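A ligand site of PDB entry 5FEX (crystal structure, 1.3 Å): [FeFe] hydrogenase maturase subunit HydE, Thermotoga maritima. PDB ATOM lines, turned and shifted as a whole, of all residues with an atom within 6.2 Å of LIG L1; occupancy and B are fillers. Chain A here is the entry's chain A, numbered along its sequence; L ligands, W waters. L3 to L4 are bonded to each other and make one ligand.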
ATOM      1  N   VAL A  72       4.153 -28.052   1.153  1.00  0.00           N
ATOM      2  CA  VAL A  72       5.529 -28.465   0.829  1.00  0.00           C
ATOM      3  C   VAL A  72       6.465 -27.447   1.416  1.00  0.00           C
ATOM      4  O   VAL A  72       6.314 -26.233   1.230  1.00  0.00           O
ATOM      5  CB  VAL A  72       5.707 -28.603  -0.671  1.00  0.00           C
ATOM      6  CG1 VAL A  72       7.202 -28.807  -1.089  1.00  0.00           C
ATOM      7  CG2 VAL A  72       4.767 -29.692  -1.215  1.00  0.00           C
ATOM      8  N   CYS A  73       7.559 -27.909   2.068  1.00  0.00           N
ATOM      9  CA  CYS A  73       8.593 -26.992   2.538  1.00  0.00           C
ATOM     10  C   CYS A  73       9.992 -27.604   2.421  1.00  0.00           C
ATOM     11  O   CYS A  73      10.227 -28.806   2.680  1.00  0.00           O
ATOM     12  CB  CYS A  73       8.382 -26.640   4.051  1.00  0.00           C
ATOM     13  SG  CYS A  73       9.368 -25.168   4.490  1.00  0.00           S
ATOM     14  N   ARG A  74      10.891 -26.734   1.982  1.00  0.00           N
ATOM     15  CA  ARG A  74      12.327 -27.055   1.870  1.00  0.00           C
ATOM     16  C   ARG A  74      13.100 -26.881   3.206  1.00  0.00           C
ATOM     17  O   ARG A  74      14.258 -27.377   3.308  1.00  0.00           O
ATOM     18  CB  ARG A  74      13.003 -26.206   0.840  1.00  0.00           C
ATOM     19  CG  ARG A  74      13.116 -24.725   1.183  1.00  0.00           C
ATOM     20  CD  ARG A  74      13.631 -23.876   0.076  1.00  0.00           C
ATOM     21  NE  ARG A  74      13.636 -22.503   0.440  1.00  0.00           N
ATOM     22  CZ  ARG A  74      14.253 -21.541  -0.191  1.00  0.00           C
ATOM     23  NH1 ARG A  74      15.032 -21.811  -1.252  1.00  0.00           N
ATOM     24  NH2 ARG A  74      14.238 -20.277   0.251  1.00  0.00           N
ATOM     25  N   LYS A  75      12.530 -26.191   4.212  1.00  0.00           N
ATOM     26  CA  LYS A  75      13.210 -25.923   5.448  1.00  0.00           C
ATOM     27  C   LYS A  75      12.838 -26.984   6.500  1.00  0.00           C
ATOM     28  O   LYS A  75      11.933 -27.794   6.292  1.00  0.00           O
ATOM     29  CB  LYS A  75      12.926 -24.482   5.945  1.00  0.00           C
ATOM     30  CG  LYS A  75      13.787 -23.450   5.268  1.00  0.00           C
ATOM     31  CD  LYS A  75      13.639 -22.074   5.839  1.00  0.00           C
ATOM     32  CE  LYS A  75      14.667 -21.044   5.408  1.00  0.00           C
ATOM     33  NZ  LYS A  75      14.875 -20.945   3.974  1.00  0.00           N
ATOM     34  N   ASN A  76      13.539 -26.949   7.622  1.00  0.00           N
ATOM     35  CA  ASN A  76      13.443 -27.988   8.642  1.00  0.00           C
ATOM     36  C   ASN A  76      13.308 -27.424  10.046  1.00  0.00           C
ATOM     37  O   ASN A  76      13.869 -27.970  11.015  1.00  0.00           O
ATOM     38  CB  ASN A  76      14.674 -28.915   8.548  1.00  0.00           C
ATOM     39  CG  ASN A  76      14.403 -30.356   8.926  1.00  0.00           C
ATOM     40  OD1 ASN A  76      13.303 -30.869   8.854  1.00  0.00           O
ATOM     41  ND2 ASN A  76      15.510 -31.080   9.279  1.00  0.00           N
ATOM     42  N   CYS A  77      12.598 -26.311  10.177  1.00  0.00           N
ATOM     43  CA  CYS A  77      12.447 -25.695  11.492  1.00  0.00           C
ATOM     44  C   CYS A  77      11.978 -26.679  12.538  1.00  0.00           C
ATOM     45  O   CYS A  77      11.081 -27.483  12.300  1.00  0.00           O
ATOM     46  CB  CYS A  77      11.457 -24.451  11.372  1.00  0.00           C
ATOM     47  SG  CYS A  77      11.829 -23.304  10.081  1.00  0.00           S
ATOM     48  N   TYR A  79      10.340 -26.627  15.272  1.00  0.00           N
ATOM     49  CA  TYR A  79       8.976 -26.510  15.899  1.00  0.00           C
ATOM     50  C   TYR A  79       7.835 -26.899  14.971  1.00  0.00           C
ATOM     51  O   TYR A  79       6.707 -27.088  15.396  1.00  0.00           O
ATOM     52  CB  TYR A  79       8.759 -25.094  16.381  1.00  0.00           C
ATOM     53  CG  TYR A  79       9.166 -24.007  15.447  1.00  0.00           C
ATOM     54  CD1 TYR A  79       8.364 -23.608  14.407  1.00  0.00           C
ATOM     55  CD2 TYR A  79      10.379 -23.340  15.578  1.00  0.00           C
ATOM     56  CE1 TYR A  79       8.775 -22.622  13.536  1.00  0.00           C
ATOM     57  CE2 TYR A  79      10.814 -22.345  14.726  1.00  0.00           C
ATOM     58  CZ  TYR A  79      10.001 -21.987  13.675  1.00  0.00           C
ATOM     59  OH  TYR A  79      10.452 -21.016  12.813  1.00  0.00           O
ATOM     60  N   CYS A  80       8.101 -26.945  13.641  1.00  0.00           N
ATOM     61  CA  CYS A  80       6.995 -26.881  12.664  1.00  0.00           C
ATOM     62  C   CYS A  80       6.602 -28.231  12.070  1.00  0.00           C
ATOM     63  O   CYS A  80       7.467 -28.991  11.562  1.00  0.00           O
ATOM     64  CB  CYS A  80       7.424 -26.026  11.493  1.00  0.00           C
ATOM     65  SG  CYS A  80       6.124 -25.748  10.238  1.00  0.00           S
ATOM     66  N   GLY A  81       5.316 -28.526  12.094  1.00  0.00           N
ATOM     67  CA  GLY A  81       4.845 -29.749  11.532  1.00  0.00           C
ATOM     68  C   GLY A  81       5.040 -29.936  10.054  1.00  0.00           C
ATOM     69  O   GLY A  81       4.916 -31.060   9.541  1.00  0.00           O
ATOM     70  N   LEU A  82       5.327 -28.865   9.300  1.00  0.00           N
ATOM     71  CA  LEU A  82       5.604 -28.924   7.898  1.00  0.00           C
ATOM     72  C   LEU A  82       7.073 -29.116   7.561  1.00  0.00           C
ATOM     73  O   LEU A  82       7.412 -29.221   6.369  1.00  0.00           O
ATOM     74  CB  LEU A  82       5.116 -27.659   7.131  1.00  0.00           C
ATOM     75  CG  LEU A  82       3.602 -27.299   7.298  1.00  0.00           C
ATOM     76  CD1 LEU A  82       3.254 -26.202   6.273  1.00  0.00           C
ATOM     77  CD2 LEU A  82       2.606 -28.465   7.338  1.00  0.00           C
ATOM     78  N   ARG A  83       7.924 -29.238   8.567  1.00  0.00           N
ATOM     79  CA  ARG A  83       9.371 -29.373   8.335  1.00  0.00           C
ATOM     80  C   ARG A  83       9.669 -30.531   7.363  1.00  0.00           C
ATOM     81  O   ARG A  83       8.992 -31.534   7.346  1.00  0.00           O
ATOM     82  CB  ARG A  83      10.127 -29.552   9.661  1.00  0.00           C
ATOM     83  CG  ARG A  83       9.798 -30.849  10.397  1.00  0.00           C
ATOM     84  CD  ARG A  83      10.226 -30.768  11.856  1.00  0.00           C
ATOM     85  NE  ARG A  83      11.602 -30.345  12.042  1.00  0.00           N
ATOM     86  CZ  ARG A  83      12.679 -31.160  12.041  1.00  0.00           C
ATOM     87  NH1 ARG A  83      12.512 -32.483  11.997  1.00  0.00           N
ATOM     88  NH2 ARG A  83      13.880 -30.624  12.161  1.00  0.00           N
ATOM     89  N   ARG A  84      10.743 -30.298   6.559  1.00  0.00           N
ATOM     90  CA  ARG A  84      11.009 -31.323   5.492  1.00  0.00           C
ATOM     91  C   ARG A  84      11.197 -32.734   5.967  1.00  0.00           C
ATOM     92  O   ARG A  84      10.820 -33.678   5.252  1.00  0.00           O
ATOM     93  CB  ARG A  84      12.132 -30.954   4.593  1.00  0.00           C
ATOM     94  CG  ARG A  84      13.454 -30.858   5.172  1.00  0.00           C
ATOM     95  CD  ARG A  84      14.563 -30.658   4.074  1.00  0.00           C
ATOM     96  NE  ARG A  84      15.774 -30.801   4.856  1.00  0.00           N
ATOM     97  CZ  ARG A  84      16.444 -29.796   5.380  1.00  0.00           C
ATOM     98  NH1 ARG A  84      16.136 -28.510   5.165  1.00  0.00           N
ATOM     99  NH2 ARG A  84      17.496 -30.048   6.166  1.00  0.00           N
ATOM    100  N   SER A 118       2.142 -20.446   2.513  1.00  0.00           N
ATOM    101  CA  SER A 118       2.601 -21.772   2.209  1.00  0.00           C
ATOM    102  C   SER A 118       3.840 -22.089   2.997  1.00  0.00           C
ATOM    103  O   SER A 118       4.503 -21.230   3.581  1.00  0.00           O
ATOM    104  CB  SER A 118       2.883 -21.959   0.720  1.00  0.00           C
ATOM    105  OG  SER A 118       3.913 -21.034   0.270  1.00  0.00           O
ATOM    106  N   GLY A 119       4.211 -23.416   2.952  1.00  0.00           N
ATOM    107  CA  GLY A 119       5.609 -23.772   3.200  1.00  0.00           C
ATOM    108  C   GLY A 119       6.495 -23.102   2.175  1.00  0.00           C
ATOM    109  O   GLY A 119       6.033 -22.538   1.171  1.00  0.00           O
ATOM    110  N   GLU A 120       7.795 -23.123   2.443  1.00  0.00           N
ATOM    111  CA  GLU A 120       8.739 -22.655   1.414  1.00  0.00           C
ATOM    112  C   GLU A 120       8.863 -23.664   0.292  1.00  0.00           C
ATOM    113  O   GLU A 120       9.771 -24.542   0.260  1.00  0.00           O
ATOM    114  CB  GLU A 120      10.127 -22.328   2.004  1.00  0.00           C
ATOM    115  CG  GLU A 120      10.145 -21.134   2.912  1.00  0.00           C
ATOM    116  CD  GLU A 120      11.515 -20.618   3.234  1.00  0.00           C
ATOM    117  OE1 GLU A 120      12.509 -21.133   2.652  1.00  0.00           O
ATOM    118  OE2 GLU A 120      11.658 -19.682   4.073  1.00  0.00           O
ATOM    119  N   GLY A 148       7.704 -17.095   3.323  1.00  0.00           N
ATOM    120  CA  GLY A 148       9.047 -17.349   3.852  1.00  0.00           C
ATOM    121  C   GLY A 148      10.107 -16.449   3.235  1.00  0.00           C
ATOM    122  O   GLY A 148       9.870 -15.375   2.754  1.00  0.00           O
ATOM    123  N   GLU A 171      10.200 -14.702  14.649  1.00  0.00           N
ATOM    124  CA  GLU A 171      10.173 -15.954  15.402  1.00  0.00           C
ATOM    125  C   GLU A 171      10.796 -15.826  16.819  1.00  0.00           C
ATOM    126  O   GLU A 171      10.130 -16.145  17.790  1.00  0.00           O
ATOM    127  CB  GLU A 171      10.808 -17.135  14.608  1.00  0.00           C
ATOM    128  CG  GLU A 171      10.295 -17.323  13.174  1.00  0.00           C
ATOM    129  CD  GLU A 171       8.836 -17.608  13.046  1.00  0.00           C
ATOM    130  OE1 GLU A 171       8.084 -17.609  14.065  1.00  0.00           O
ATOM    131  OE2 GLU A 171       8.403 -17.825  11.845  1.00  0.00           O
ATOM    132  N   ARG A 182      16.084 -22.997  13.711  1.00  0.00           N
ATOM    133  CA  ARG A 182      15.862 -22.754  12.272  1.00  0.00           C
ATOM    134  C   ARG A 182      17.235 -22.981  11.557  1.00  0.00           C
ATOM    135  O   ARG A 182      17.911 -22.074  11.153  1.00  0.00           O
ATOM    136  CB  ARG A 182      15.286 -21.376  12.013  1.00  0.00           C
ATOM    137  CG  ARG A 182      14.065 -21.094  12.877  1.00  0.00           C
ATOM    138  CD  ARG A 182      13.330 -19.797  12.522  1.00  0.00           C
ATOM    139  NE  ARG A 182      12.723 -19.976  11.194  1.00  0.00           N
ATOM    140  CZ  ARG A 182      13.101 -19.354  10.068  1.00  0.00           C
ATOM    141  NH1 ARG A 182      13.946 -18.379  10.058  1.00  0.00           N
ATOM    142  NH2 ARG A 182      12.549 -19.807   8.935  1.00  0.00           N
ATOM    143  N   ARG A 190      16.803 -13.447   8.399  1.00  0.00           N
ATOM    144  CA  ARG A 190      15.393 -13.110   8.635  1.00  0.00           C
ATOM    145  C   ARG A 190      15.158 -11.621   8.667  1.00  0.00           C
ATOM    146  O   ARG A 190      14.266 -11.057   8.036  1.00  0.00           O
ATOM    147  CB  ARG A 190      14.927 -13.795   9.921  1.00  0.00           C
ATOM    148  CG  ARG A 190      13.400 -13.890  10.083  1.00  0.00           C
ATOM    149  CD  ARG A 190      12.842 -14.999   9.194  1.00  0.00           C
ATOM    150  NE  ARG A 190      11.475 -15.354   9.539  1.00  0.00           N
ATOM    151  CZ  ARG A 190      10.750 -16.258   8.867  1.00  0.00           C
ATOM    152  NH1 ARG A 190      11.310 -16.987   7.908  1.00  0.00           N
ATOM    153  NH2 ARG A 190       9.490 -16.478   9.214  1.00  0.00           N
ATOM    154  N   TYR A 313      -2.636 -29.029   6.619  1.00  0.00           N
ATOM    155  CA  TYR A 313      -1.789 -27.907   6.931  1.00  0.00           C
ATOM    156  C   TYR A 313      -1.777 -27.683   8.442  1.00  0.00           C
ATOM    157  O   TYR A 313      -2.524 -26.827   8.946  1.00  0.00           O
ATOM    158  CB  TYR A 313      -2.253 -26.660   6.158  1.00  0.00           C
ATOM    159  CG  TYR A 313      -1.210 -25.567   6.064  1.00  0.00           C
ATOM    160  CD1 TYR A 313      -0.393 -25.456   4.918  1.00  0.00           C
ATOM    161  CD2 TYR A 313      -1.071 -24.616   7.045  1.00  0.00           C
ATOM    162  CE1 TYR A 313       0.523 -24.462   4.792  1.00  0.00           C
ATOM    163  CE2 TYR A 313      -0.193 -23.570   6.918  1.00  0.00           C
ATOM    164  CZ  TYR A 313       0.603 -23.484   5.767  1.00  0.00           C
ATOM    165  OH  TYR A 313       1.470 -22.423   5.556  1.00  0.00           O
ATOM    166  N   LEU A 315       0.666 -26.814  11.266  1.00  0.00           N
ATOM    167  CA  LEU A 315       1.923 -26.373  11.796  1.00  0.00           C
ATOM    168  C   LEU A 315       2.055 -26.884  13.178  1.00  0.00           C
ATOM    169  O   LEU A 315       3.158 -27.193  13.603  1.00  0.00           O
ATOM    170  CB  LEU A 315       1.965 -24.825  11.802  1.00  0.00           C
ATOM    171  CG  LEU A 315       1.630 -24.053  10.503  1.00  0.00           C
ATOM    172  CD1 LEU A 315       1.882 -22.626  10.712  1.00  0.00           C
ATOM    173  CD2 LEU A 315       2.327 -24.586   9.389  1.00  0.00           C
HETATM  174 FE1  LIG L   1       7.390 -24.498   8.809  1.00  0.00          FE
HETATM  175 FE2  LIG L   1       8.794 -24.405   6.513  1.00  0.00          FE
HETATM  176 FE3  LIG L   1       9.847 -23.354   8.810  1.00  0.00          FE
HETATM  177 FE4  LIG L   1       7.568 -21.931   7.600  1.00  0.00          FE
HETATM  178  S1  LIG L   1       9.852 -22.335   6.766  1.00  0.00           S
HETATM  179  S2  LIG L   1       7.941 -22.524   9.850  1.00  0.00           S
HETATM  180  S3  LIG L   1       6.567 -23.955   6.803  1.00  0.00           S
HETATM  181  S4  LIG L   1       9.400 -25.578   8.355  1.00  0.00           S
HETATM  182  N1  LG2 L   2       6.929 -20.777   5.777  1.00  0.00           N
HETATM  183  C1  LG2 L   2       6.576 -19.319   5.969  1.00  0.00           C
HETATM  184  C2  LG2 L   2       7.364 -18.829   7.151  1.00  0.00           C
HETATM  185  O1  LG2 L   2       7.470 -17.605   7.363  1.00  0.00           O
HETATM  186  C3  LG2 L   2       5.095 -19.204   6.254  1.00  0.00           C
HETATM  187  C4  LG2 L   2       4.615 -19.426   7.726  1.00  0.00           C
HETATM  188  S1  LG2 L   2       4.918 -21.075   8.344  1.00  0.00           S
HETATM  189  C5  LG2 L   2       3.789 -21.993   7.354  1.00  0.00           C
HETATM  190  O2  LG2 L   2       7.913 -19.736   7.926  1.00  0.00           O
HETATM  191  N1  LG3 L   3       3.385 -23.671  17.308  1.00  0.00           N
HETATM  192  C1  LG3 L   3       2.866 -22.468  17.103  1.00  0.00           C
HETATM  193  N2  LG3 L   3       3.122 -21.664  16.110  1.00  0.00           N
HETATM  194  C2  LG3 L   3       3.803 -22.173  15.096  1.00  0.00           C
HETATM  195  N3  LG3 L   3       4.242 -21.653  13.949  1.00  0.00           N
HETATM  196  C3  LG3 L   3       4.953 -22.620  13.284  1.00  0.00           C
HETATM  197  N4  LG3 L   3       5.013 -23.792  13.986  1.00  0.00           N
HETATM  198  C4  LG3 L   3       4.324 -23.513  15.142  1.00  0.00           C
HETATM  199  C5  LG3 L   3       4.033 -24.284  16.306  1.00  0.00           C
HETATM  200  N5  LG3 L   3       4.519 -25.560  16.447  1.00  0.00           N
HETATM  201  C6  LG3 L   3       4.116 -20.225  13.659  1.00  0.00           C
HETATM  202  C7  LG3 L   3       5.482 -19.586  13.277  1.00  0.00           C
HETATM  203  C8  LG3 L   3       5.226 -19.160  11.836  1.00  0.00           C
HETATM  204  C9  LG3 L   3       3.702 -18.754  11.935  1.00  0.00           C
HETATM  205  C10 LG3 L   3       2.891 -18.678  10.675  1.00  0.00           C
HETATM  206  O1  LG3 L   3       3.192 -19.960  12.649  1.00  0.00           O
HETATM  207  O2  LG3 L   3       5.610 -18.447  14.160  1.00  0.00           O
HETATM  208  O3  LG3 L   3       5.892 -17.947  11.450  1.00  0.00           O
HETATM  209  N1  LG4 L   4      -1.470 -17.055  12.746  1.00  0.00           N
HETATM  210  C1  LG4 L   4      -1.231 -18.471  12.391  1.00  0.00           C
HETATM  211  C2  LG4 L   4       0.218 -18.827  12.263  1.00  0.00           C
HETATM  212 SE1  LG4 L   4       1.121 -17.631  10.952  1.00  0.00          SE
HETATM  213  C3  LG4 L   4      -1.775 -19.292  13.475  1.00  0.00           C
HETATM  214  O1  LG4 L   4      -1.801 -18.932  14.689  1.00  0.00           O
HETATM  215  O2  LG4 L   4      -2.197 -20.409  13.106  1.00  0.00           O
HETATM  216  O   HOH W   1      10.443 -19.172   6.427  1.00  0.00           O
HETATM  217  O   HOH W   2       9.652 -19.863  10.518  1.00  0.00           O
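The guanidinium group (NH2) of Arg 190 is in salt-bridge range of an oxygen (O1) of LG2 L2 (3.0 Å).
FE3 of LIG L1 is bound by SG of Cys 77.
The backbone carbonyl oxygen of Tyr 79 sits at hydrogen-bond distance from a nitrogen (N5) of LG3 L3 (2.9 Å).
N of Cys 77 sits close to S4 of LIG L1, 3.8 Å away.
A nitrogen (N1) of LG2 L2 sits close to the backbone carbonyl oxygen (O) of Ser 118 (3.3 Å).
The side-chain sulfur (SG) of Cys 73 is bound to an iron atom (FE2) of LIG L1 (2.2 Å).
The side-chain carboxylate (OE2) of Glu 171 lies within hydrogen-bond range of an oxygen (O3) of LG3 L3 (2.5 Å).
An iron atom (FE1) of LIG L1 is bound by the side-chain sulfur of Cys 80 (2.3 Å).
An oxygen (O2) of LG2 L2 binds an iron atom (FE4) of LIG L1.
The backbone NH (N) of Leu 82 lies close to the side-chain sulfur (SG) of Cys 80, 3.4 Å away.
The side-chain hydroxyl (OH) of Tyr 79 lies within hydrogen-bond range of the guanidinium group (NE) of Arg 182 (3.0 Å).
O of Cys 77 sits at hydrogen-bond distance from NE of Arg 83.
The side-chain sulfur of Cys 73 lies close to the backbone NH of Lys 75 (3.3 Å).
NE of Arg 182 sits close to SG of Cys 77 (3.6 Å).
OE1 of Glu 120 lies within salt-bridge range of NZ of Lys 75 (2.7 Å).
The side-chain sulfur (SG) of Cys 73 sits close to the backbone NH (N) of Glu 120.
The backbone carbonyl oxygen (O) of Asn 76 lies within hydrogen-bond range of the guanidinium group (NH2) of Arg 83 (2.9 Å).
Lys 75 touches LIG L1.
Tyr 79 touches LIG L1.
Leu 82 touches LIG L1 (CB to S3, 3.99 Å).
Arg 83 touches LIG L1.
Gly 119 touches LIG L1.
Hydrophobic or aromatic side chains that line LIG L1: Tyr 79 and Leu 82.
Water W2 lies within hydrogen-bond range of the side-chain hydroxyl (OH) of Tyr 79 (2.7 Å), the side-chain carboxylate (OE2) of Glu 171 (2.7 Å), the guanidinium group (NE) of Arg 182 (3.1 Å) and a sulfur (S2) of LIG L1 (3.2 Å).
Water W1 lies within hydrogen-bond range of the side-chain carboxylate (OE2) of Glu 120, the guanidinium group (NH1) of Arg 190, a sulfur (S1) of LIG L1, the guanidinium group (NH2) of Arg 182 and an oxygen (O1) of LG2 L2.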
